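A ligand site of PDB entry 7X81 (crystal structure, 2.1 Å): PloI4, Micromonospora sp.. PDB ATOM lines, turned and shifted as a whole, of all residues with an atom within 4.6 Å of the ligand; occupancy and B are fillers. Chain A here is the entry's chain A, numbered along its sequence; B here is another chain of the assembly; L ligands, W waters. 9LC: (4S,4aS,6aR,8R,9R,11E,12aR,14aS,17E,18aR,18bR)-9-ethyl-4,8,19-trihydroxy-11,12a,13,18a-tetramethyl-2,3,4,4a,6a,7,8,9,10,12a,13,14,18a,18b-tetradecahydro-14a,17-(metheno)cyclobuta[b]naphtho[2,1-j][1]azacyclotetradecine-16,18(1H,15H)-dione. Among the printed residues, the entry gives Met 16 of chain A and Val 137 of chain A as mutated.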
ATOM      1  N   MET A  16     -17.724  -2.766 -37.664  1.00  0.00           N
ATOM      2  CA  MET A  16     -17.567  -3.319 -36.326  1.00  0.00           C
ATOM      3  C   MET A  16     -18.925  -3.526 -35.643  1.00  0.00           C
ATOM      4  O   MET A  16     -19.747  -2.602 -35.581  1.00  0.00           O
ATOM      5  CB  MET A  16     -16.672  -2.388 -35.506  1.00  0.00           C
ATOM      6  CG  MET A  16     -16.422  -2.852 -34.084  1.00  0.00           C
ATOM      7  SD  MET A  16     -15.178  -1.818 -33.311  1.00  0.00           S
ATOM      8  CE  MET A  16     -13.726  -2.098 -34.378  1.00  0.00           C
ATOM      9  N   THR A  18     -20.618  -4.020 -32.174  1.00  0.00           N
ATOM     10  CA  THR A  18     -20.288  -3.665 -30.802  1.00  0.00           C
ATOM     11  C   THR A  18     -21.353  -4.139 -29.845  1.00  0.00           C
ATOM     12  O   THR A  18     -22.520  -3.726 -29.978  1.00  0.00           O
ATOM     13  CB  THR A  18     -20.186  -2.164 -30.665  1.00  0.00           C
ATOM     14  OG1 THR A  18     -21.484  -1.603 -30.936  1.00  0.00           O
ATOM     15  CG2 THR A  18     -19.140  -1.601 -31.563  1.00  0.00           C
ATOM     16  N   ILE A  20     -22.280  -3.678 -26.073  1.00  0.00           N
ATOM     17  CA  ILE A  20     -21.958  -2.669 -25.079  1.00  0.00           C
ATOM     18  C   ILE A  20     -22.669  -3.000 -23.784  1.00  0.00           C
ATOM     19  O   ILE A  20     -23.880  -3.289 -23.792  1.00  0.00           O
ATOM     20  CB  ILE A  20     -22.343  -1.279 -25.563  1.00  0.00           C
ATOM     21  CG1 ILE A  20     -21.608  -0.937 -26.849  1.00  0.00           C
ATOM     22  CG2 ILE A  20     -21.986  -0.227 -24.517  1.00  0.00           C
ATOM     23  CD1 ILE A  20     -22.028   0.402 -27.442  1.00  0.00           C
ATOM     24  N   VAL A  42     -17.009  -2.599 -24.211  1.00  0.00           N
ATOM     25  CA  VAL A  42     -17.369  -2.831 -25.600  1.00  0.00           C
ATOM     26  C   VAL A  42     -16.675  -4.125 -26.063  1.00  0.00           C
ATOM     27  O   VAL A  42     -15.448  -4.146 -26.221  1.00  0.00           O
ATOM     28  CB  VAL A  42     -16.949  -1.675 -26.519  1.00  0.00           C
ATOM     29  CG1 VAL A  42     -17.461  -1.908 -27.915  1.00  0.00           C
ATOM     30  CG2 VAL A  42     -17.556  -0.331 -26.019  1.00  0.00           C
ATOM     31  N   PHE A  44     -16.250  -6.445 -29.179  1.00  0.00           N
ATOM     32  CA  PHE A  44     -16.457  -6.170 -30.589  1.00  0.00           C
ATOM     33  C   PHE A  44     -15.874  -7.226 -31.490  1.00  0.00           C
ATOM     34  O   PHE A  44     -14.929  -7.934 -31.115  1.00  0.00           O
ATOM     35  CB  PHE A  44     -15.879  -4.809 -30.984  1.00  0.00           C
ATOM     36  CG  PHE A  44     -14.383  -4.679 -30.863  1.00  0.00           C
ATOM     37  CD1 PHE A  44     -13.567  -5.004 -31.944  1.00  0.00           C
ATOM     38  CD2 PHE A  44     -13.808  -4.165 -29.728  1.00  0.00           C
ATOM     39  CE1 PHE A  44     -12.187  -4.821 -31.856  1.00  0.00           C
ATOM     40  CE2 PHE A  44     -12.462  -3.966 -29.634  1.00  0.00           C
ATOM     41  CZ  PHE A  44     -11.642  -4.330 -30.704  1.00  0.00           C
ATOM     42  N   SER A  63     -12.794  -3.364 -25.215  1.00  0.00           N
ATOM     43  CA  SER A  63     -12.447  -2.067 -24.662  1.00  0.00           C
ATOM     44  C   SER A  63     -13.251  -1.849 -23.370  1.00  0.00           C
ATOM     45  O   SER A  63     -14.414  -2.271 -23.273  1.00  0.00           O
ATOM     46  CB  SER A  63     -12.762  -0.913 -25.620  1.00  0.00           C
ATOM     47  OG  SER A  63     -11.832  -0.847 -26.686  1.00  0.00           O
ATOM     48  N   ILE A  65     -13.865   1.347 -20.219  1.00  0.00           N
ATOM     49  CA  ILE A  65     -13.673   2.753 -19.851  1.00  0.00           C
ATOM     50  C   ILE A  65     -13.155   2.836 -18.414  1.00  0.00           C
ATOM     51  O   ILE A  65     -13.623   2.130 -17.526  1.00  0.00           O
ATOM     52  CB  ILE A  65     -14.984   3.573 -20.015  1.00  0.00           C
ATOM     53  CG1 ILE A  65     -15.517   3.400 -21.440  1.00  0.00           C
ATOM     54  CG2 ILE A  65     -14.769   5.017 -19.601  1.00  0.00           C
ATOM     55  CD1 ILE A  65     -16.764   4.291 -21.784  1.00  0.00           C
ATOM     56  N   GLN A  75     -10.014   4.788 -22.418  1.00  0.00           N
ATOM     57  CA  GLN A  75     -10.422   3.416 -22.686  1.00  0.00           C
ATOM     58  C   GLN A  75      -9.165   2.568 -22.796  1.00  0.00           C
ATOM     59  O   GLN A  75      -8.133   3.037 -23.240  1.00  0.00           O
ATOM     60  CB  GLN A  75     -11.277   3.287 -23.959  1.00  0.00           C
ATOM     61  CG  GLN A  75     -12.563   4.103 -23.889  1.00  0.00           C
ATOM     62  CD  GLN A  75     -13.536   3.857 -25.044  1.00  0.00           C
ATOM     63  OE1 GLN A  75     -13.301   3.021 -25.876  1.00  0.00           O
ATOM     64  NE2 GLN A  75     -14.654   4.555 -25.046  1.00  0.00           N
ATOM     65  N   VAL A  77      -7.871  -1.153 -24.410  1.00  0.00           N
ATOM     66  CA  VAL A  77      -8.271  -2.200 -25.350  1.00  0.00           C
ATOM     67  C   VAL A  77      -7.234  -3.304 -25.369  1.00  0.00           C
ATOM     68  O   VAL A  77      -6.033  -3.059 -25.244  1.00  0.00           O
ATOM     69  CB  VAL A  77      -8.475  -1.638 -26.767  1.00  0.00           C
ATOM     70  CG1 VAL A  77      -7.172  -1.090 -27.280  1.00  0.00           C
ATOM     71  CG2 VAL A  77      -8.997  -2.692 -27.700  1.00  0.00           C
ATOM     72  N   TRP A  91      -3.004  -6.020 -30.831  1.00  0.00           N
ATOM     73  CA  TRP A  91      -2.885  -4.598 -30.505  1.00  0.00           C
ATOM     74  C   TRP A  91      -3.602  -4.310 -29.196  1.00  0.00           C
ATOM     75  O   TRP A  91      -4.687  -4.850 -28.919  1.00  0.00           O
ATOM     76  CB  TRP A  91      -3.396  -3.696 -31.646  1.00  0.00           C
ATOM     77  CG  TRP A  91      -4.746  -4.040 -32.311  1.00  0.00           C
ATOM     78  CD1 TRP A  91      -4.955  -4.932 -33.283  1.00  0.00           C
ATOM     79  CD2 TRP A  91      -6.012  -3.391 -32.108  1.00  0.00           C
ATOM     80  NE1 TRP A  91      -6.248  -4.918 -33.706  1.00  0.00           N
ATOM     81  CE2 TRP A  91      -6.941  -3.998 -32.985  1.00  0.00           C
ATOM     82  CE3 TRP A  91      -6.467  -2.395 -31.241  1.00  0.00           C
ATOM     83  CZ2 TRP A  91      -8.310  -3.649 -33.006  1.00  0.00           C
ATOM     84  CZ3 TRP A  91      -7.811  -2.039 -31.296  1.00  0.00           C
ATOM     85  CH2 TRP A  91      -8.705  -2.658 -32.165  1.00  0.00           C
ATOM     86  N   TYR A  95      -6.131   4.712 -24.581  1.00  0.00           N
ATOM     87  CA  TYR A  95      -6.249   5.927 -25.375  1.00  0.00           C
ATOM     88  C   TYR A  95      -7.264   6.828 -24.684  1.00  0.00           C
ATOM     89  O   TYR A  95      -8.152   6.343 -23.963  1.00  0.00           O
ATOM     90  CB  TYR A  95      -6.669   5.653 -26.835  1.00  0.00           C
ATOM     91  CG  TYR A  95      -7.775   4.650 -26.945  1.00  0.00           C
ATOM     92  CD1 TYR A  95      -7.524   3.310 -26.844  1.00  0.00           C
ATOM     93  CD2 TYR A  95      -9.101   5.063 -27.172  1.00  0.00           C
ATOM     94  CE1 TYR A  95      -8.525   2.394 -26.921  1.00  0.00           C
ATOM     95  CE2 TYR A  95     -10.118   4.140 -27.305  1.00  0.00           C
ATOM     96  CZ  TYR A  95      -9.816   2.805 -27.151  1.00  0.00           C
ATOM     97  OH  TYR A  95     -10.786   1.863 -27.195  1.00  0.00           O
ATOM     98  N   THR A  96      -7.096   8.143 -24.893  1.00  0.00           N
ATOM     99  CA  THR A  96      -8.029   9.146 -24.400  1.00  0.00           C
ATOM    100  C   THR A  96      -9.390   9.023 -25.066  1.00  0.00           C
ATOM    101  O   THR A  96      -9.507   8.856 -26.290  1.00  0.00           O
ATOM    102  CB  THR A  96      -7.444  10.524 -24.660  1.00  0.00           C
ATOM    103  OG1 THR A  96      -6.218  10.619 -23.929  1.00  0.00           O
ATOM    104  CG2 THR A  96      -8.374  11.622 -24.193  1.00  0.00           C
ATOM    105  N   MET A  97     -10.437   9.119 -24.253  1.00  0.00           N
ATOM    106  CA  MET A  97     -11.755   8.892 -24.814  1.00  0.00           C
ATOM    107  C   MET A  97     -12.244  10.098 -25.606  1.00  0.00           C
ATOM    108  O   MET A  97     -12.773   9.943 -26.705  1.00  0.00           O
ATOM    109  CB  MET A  97     -12.751   8.540 -23.728  1.00  0.00           C
ATOM    110  CG  MET A  97     -14.113   8.337 -24.284  1.00  0.00           C
ATOM    111  SD  MET A  97     -15.161   7.359 -23.220  1.00  0.00           S
ATOM    112  CE  MET A  97     -16.649   7.380 -24.244  1.00  0.00           C
ATOM    113  N   THR A 100     -14.580  11.862 -29.068  1.00  0.00           N
ATOM    114  CA  THR A 100     -14.754  10.501 -29.531  1.00  0.00           C
ATOM    115  C   THR A 100     -14.551  10.319 -31.018  1.00  0.00           C
ATOM    116  O   THR A 100     -14.480   9.168 -31.459  1.00  0.00           O
ATOM    117  CB  THR A 100     -16.157   9.973 -29.182  1.00  0.00           C
ATOM    118  OG1 THR A 100     -17.140  10.887 -29.662  1.00  0.00           O
ATOM    119  CG2 THR A 100     -16.281   9.853 -27.738  1.00  0.00           C
ATOM    120  N   LYS A 104      -7.579   7.474 -32.868  1.00  0.00           N
ATOM    121  CA  LYS A 104      -6.987   6.860 -31.703  1.00  0.00           C
ATOM    122  C   LYS A 104      -5.954   5.861 -32.185  1.00  0.00           C
ATOM    123  O   LYS A 104      -6.016   5.389 -33.323  1.00  0.00           O
ATOM    124  CB  LYS A 104      -8.050   6.150 -30.851  1.00  0.00           C
ATOM    125  CG  LYS A 104      -9.293   7.015 -30.585  1.00  0.00           C
ATOM    126  CD  LYS A 104      -9.004   8.237 -29.697  1.00  0.00           C
ATOM    127  CE  LYS A 104     -10.310   9.031 -29.509  1.00  0.00           C
ATOM    128  NZ  LYS A 104     -10.108  10.140 -28.611  1.00  0.00           N
ATOM    129  N   PHE A 124      -7.467   3.700 -35.332  1.00  0.00           N
ATOM    130  CA  PHE A 124      -8.889   3.542 -35.592  1.00  0.00           C
ATOM    131  C   PHE A 124      -9.541   4.871 -35.275  1.00  0.00           C
ATOM    132  O   PHE A 124      -9.148   5.566 -34.333  1.00  0.00           O
ATOM    133  CB  PHE A 124      -9.516   2.429 -34.753  1.00  0.00           C
ATOM    134  CG  PHE A 124      -8.958   2.336 -33.352  1.00  0.00           C
ATOM    135  CD1 PHE A 124      -7.765   1.669 -33.094  1.00  0.00           C
ATOM    136  CD2 PHE A 124      -9.653   2.866 -32.281  1.00  0.00           C
ATOM    137  CE1 PHE A 124      -7.268   1.572 -31.804  1.00  0.00           C
ATOM    138  CE2 PHE A 124      -9.175   2.756 -30.994  1.00  0.00           C
ATOM    139  CZ  PHE A 124      -7.975   2.130 -30.755  1.00  0.00           C
ATOM    140  N   LEU A 126     -13.646   6.616 -35.443  1.00  0.00           N
ATOM    141  CA  LEU A 126     -15.067   6.395 -35.656  1.00  0.00           C
ATOM    142  C   LEU A 126     -15.585   7.351 -36.693  1.00  0.00           C
ATOM    143  O   LEU A 126     -15.429   8.557 -36.561  1.00  0.00           O
ATOM    144  CB  LEU A 126     -15.837   6.587 -34.359  1.00  0.00           C
ATOM    145  CG  LEU A 126     -17.355   6.392 -34.415  1.00  0.00           C
ATOM    146  CD1 LEU A 126     -17.691   4.939 -34.675  1.00  0.00           C
ATOM    147  CD2 LEU A 126     -18.028   6.878 -33.120  1.00  0.00           C
ATOM    148  N   ARG A 129     -22.151   5.718 -36.619  1.00  0.00           N
ATOM    149  CA  ARG A 129     -22.842   4.689 -35.834  1.00  0.00           C
ATOM    150  C   ARG A 129     -24.203   4.522 -36.473  1.00  0.00           C
ATOM    151  O   ARG A 129     -25.169   5.173 -36.079  1.00  0.00           O
ATOM    152  CB  ARG A 129     -22.897   5.054 -34.360  1.00  0.00           C
ATOM    153  CG  ARG A 129     -21.639   4.512 -33.752  1.00  0.00           C
ATOM    154  CD  ARG A 129     -21.436   4.610 -32.340  1.00  0.00           C
ATOM    155  NE  ARG A 129     -22.283   3.809 -31.485  1.00  0.00           N
ATOM    156  CZ  ARG A 129     -22.305   2.491 -31.333  1.00  0.00           C
ATOM    157  NH1 ARG A 129     -23.121   2.039 -30.393  1.00  0.00           N
ATOM    158  NH2 ARG A 129     -21.562   1.629 -32.038  1.00  0.00           N
ATOM    159  N   SER A 135     -20.478   0.179 -35.597  1.00  0.00           N
ATOM    160  CA  SER A 135     -19.568   1.294 -35.757  1.00  0.00           C
ATOM    161  C   SER A 135     -18.887   1.142 -37.101  1.00  0.00           C
ATOM    162  O   SER A 135     -18.438   0.061 -37.436  1.00  0.00           O
ATOM    163  CB  SER A 135     -18.560   1.336 -34.615  1.00  0.00           C
ATOM    164  OG  SER A 135     -19.205   1.579 -33.382  1.00  0.00           O
ATOM    165  N   VAL A 137     -15.667   2.339 -38.901  1.00  0.00           N
ATOM    166  CA  VAL A 137     -14.387   2.816 -38.391  1.00  0.00           C
ATOM    167  C   VAL A 137     -13.404   2.939 -39.552  1.00  0.00           C
ATOM    168  O   VAL A 137     -13.383   2.082 -40.438  1.00  0.00           O
ATOM    169  CB  VAL A 137     -13.855   1.839 -37.305  1.00  0.00           C
ATOM    170  CG1 VAL A 137     -12.535   2.310 -36.723  1.00  0.00           C
ATOM    171  CG2 VAL A 137     -14.929   1.612 -36.195  1.00  0.00           C
ATOM    172  N   LEU B  34     -22.900  10.945 -21.101  1.00  0.00           N
ATOM    173  CA  LEU B  34     -22.992   9.699 -21.839  1.00  0.00           C
ATOM    174  C   LEU B  34     -23.315   8.571 -20.886  1.00  0.00           C
ATOM    175  O   LEU B  34     -23.076   8.675 -19.678  1.00  0.00           O
ATOM    176  CB  LEU B  34     -21.676   9.408 -22.565  1.00  0.00           C
ATOM    177  CG  LEU B  34     -21.232  10.302 -23.724  1.00  0.00           C
ATOM    178  CD1 LEU B  34     -19.893   9.742 -24.297  1.00  0.00           C
ATOM    179  CD2 LEU B  34     -22.272  10.310 -24.796  1.00  0.00           C
ATOM    180  N   PRO B  35     -23.848   7.494 -21.385  1.00  0.00           N
ATOM    181  CA  PRO B  35     -24.225   6.371 -20.464  1.00  0.00           C
ATOM    182  C   PRO B  35     -23.026   5.497 -20.142  1.00  0.00           C
ATOM    183  O   PRO B  35     -22.821   4.414 -20.689  1.00  0.00           O
ATOM    184  CB  PRO B  35     -25.263   5.591 -21.290  1.00  0.00           C
ATOM    185  CG  PRO B  35     -24.723   5.738 -22.702  1.00  0.00           C
ATOM    186  CD  PRO B  35     -24.296   7.230 -22.764  1.00  0.00           C
ATOM    187  N   ILE B  36     -22.178   5.954 -19.231  1.00  0.00           N
ATOM    188  CA  ILE B  36     -20.979   5.207 -18.922  1.00  0.00           C
ATOM    189  C   ILE B  36     -20.639   5.248 -17.441  1.00  0.00           C
ATOM    190  O   ILE B  36     -21.059   6.111 -16.687  1.00  0.00           O
ATOM    191  CB  ILE B  36     -19.787   5.725 -19.770  1.00  0.00           C
ATOM    192  CG1 ILE B  36     -19.387   7.157 -19.422  1.00  0.00           C
ATOM    193  CG2 ILE B  36     -20.101   5.677 -21.287  1.00  0.00           C
ATOM    194  CD1 ILE B  36     -18.575   7.825 -20.547  1.00  0.00           C
HETATM  195  CG  9LC L   1     -18.139   3.671 -28.581  1.00  0.00           C
HETATM  196  O5  9LC L   1     -21.584   6.590 -26.300  1.00  0.00           O
HETATM  197  CD2 9LC L   1     -17.911   4.935 -29.437  1.00  0.00           C
HETATM  198  CE1 9LC L   1     -19.972   5.124 -27.409  1.00  0.00           C
HETATM  199  CE2 9LC L   1     -18.998   5.835 -29.549  1.00  0.00           C
HETATM  200  CZ  9LC L   1     -19.898   6.023 -28.482  1.00  0.00           C
HETATM  201  C1  9LC L   1     -20.370   5.882 -26.113  1.00  0.00           C
HETATM  202  C11 9LC L   1     -12.962   0.775 -32.164  1.00  0.00           C
HETATM  203  C14 9LC L   1     -18.705   4.204 -27.213  1.00  0.00           C
HETATM  204  C15 9LC L   1     -16.188   2.160 -29.357  1.00  0.00           C
HETATM  205  C16 9LC L   1     -16.550   1.611 -30.563  1.00  0.00           C
HETATM  206  C18 9LC L   1     -16.632   5.756 -29.154  1.00  0.00           C
HETATM  207  C19 9LC L   1     -15.452   5.403 -30.026  1.00  0.00           C
HETATM  208  C2  9LC L   1     -20.540   4.933 -24.907  1.00  0.00           C
HETATM  209  C20 9LC L   1     -13.997   5.333 -29.435  1.00  0.00           C
HETATM  210  C21 9LC L   1     -13.799   6.675 -28.674  1.00  0.00           C
HETATM  211  C22 9LC L   1     -12.890   4.967 -30.466  1.00  0.00           C
HETATM  212  C23 9LC L   1     -12.612   6.710 -27.673  1.00  0.00           C
HETATM  213  C24 9LC L   1     -13.194   3.726 -31.104  1.00  0.00           C
HETATM  214  C26 9LC L   1     -12.959   2.506 -30.438  1.00  0.00           C
HETATM  215  C27 9LC L   1     -13.234   1.142 -30.721  1.00  0.00           C
HETATM  216  C28 9LC L   1     -14.626   0.631 -30.039  1.00  0.00           C
HETATM  217  C29 9LC L   1     -12.648   0.151 -29.739  1.00  0.00           C
HETATM  218  C3  9LC L   1     -19.359   3.974 -24.678  1.00  0.00           C
HETATM  219  C30 9LC L   1     -15.124   1.388 -28.969  1.00  0.00           C
HETATM  220  C33 9LC L   1     -13.939  -0.698 -29.792  1.00  0.00           C
HETATM  221  C4  9LC L   1     -18.925   3.285 -25.996  1.00  0.00           C
HETATM  222  C5  9LC L   1     -13.667   3.810 -32.378  1.00  0.00           C
HETATM  223  C6  9LC L   1     -16.905   2.928 -28.408  1.00  0.00           C
HETATM  224  C7  9LC L   1     -19.266   2.859 -29.138  1.00  0.00           C
HETATM  225  C8  9LC L   1     -11.394  -0.550 -30.192  1.00  0.00           C
HETATM  226  N5N 9LC L   1     -15.743   0.660 -30.999  1.00  0.00           N
HETATM  227  O31 9LC L   1     -16.368   3.074 -27.278  1.00  0.00           O
HETATM  228  O32 9LC L   1     -17.609   1.916 -31.361  1.00  0.00           O
HETATM  229  O34 9LC L   1     -14.401   1.481 -27.798  1.00  0.00           O
HETATM  230  O4  9LC L   1     -15.371   6.179 -31.279  1.00  0.00           O
HETATM  231  O   HOH W   1     -21.211   9.238 -28.310  1.00  0.00           O
HETATM  232  O   HOH W   2     -23.995   5.679 -26.190  1.00  0.00           O
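O34 of the ligand lies within hydrogen-bond range of OE1 of Gln 75 (2.7 Å). OG of Ser 135 lies within hydrogen-bond range of O32 of the ligand (2.6 Å). The backbone carbonyl oxygen of Thr 100 lies within hydrogen-bond range of an oxygen (O4) of the ligand, 3.1 Å away. SD of Met 16 sits at hydrogen-bond distance from N5N of the ligand (3.4 Å).
Merely in contact with the ligand: Leu 126, Ser 63, Met 97, Phe 44, Tyr 95, Ile 36 of chain B, Lys 104, Arg 129, Phe 124, Val 42, Thr 18, Ile 65 and Trp 91. Hydrophobic or aromatic side chains that line the ligand: Met 16, Val 42, Phe 44, Ile 65, Trp 91, Tyr 95, Phe 124, Leu 126 and Ile 36 of chain B. Within 4 Å of the ligand: Met 16, Thr 18, Val 42, Phe 44, Ser 63, Ile 65, Gln 75, Trp 91, Tyr 95, Met 97, Thr 100, Lys 104, Phe 124, Leu 126, Arg 129, Ser 135 and Ile 36 of chain B. The nearest printed residue that does not touch the ligand is Thr 96 (4.02 Å).
O of Tyr 95 sits at hydrogen-bond distance from N of Gln 75, at 2.9 Å. The backbone carbonyl oxygen (O) of Phe 124 sits at hydrogen-bond distance from the backbone NH (N) of Lys 104 (2.9 Å). The backbone NH of Ser 135 sits at hydrogen-bond distance from the backbone carbonyl oxygen of Met 16. NZ of Lys 104 lies within hydrogen-bond range of O of Thr 96 (2.7 Å). The backbone carbonyl oxygen (O) of Ser 63 sits at hydrogen-bond distance from the backbone NH (N) of Val 42 (2.8 Å). OG of Ser 135 lies within hydrogen-bond range of NH2 of Arg 129, 2.7 Å away. The side-chain sulfur of Met 97 is in hydrogen-bond range of the side-chain amide nitrogen of Gln 75, at 3.4 Å. The backbone carbonyl oxygen of Met 97 sits at hydrogen-bond distance from the side-chain amino group of Lys 104, at 3.3 Å.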
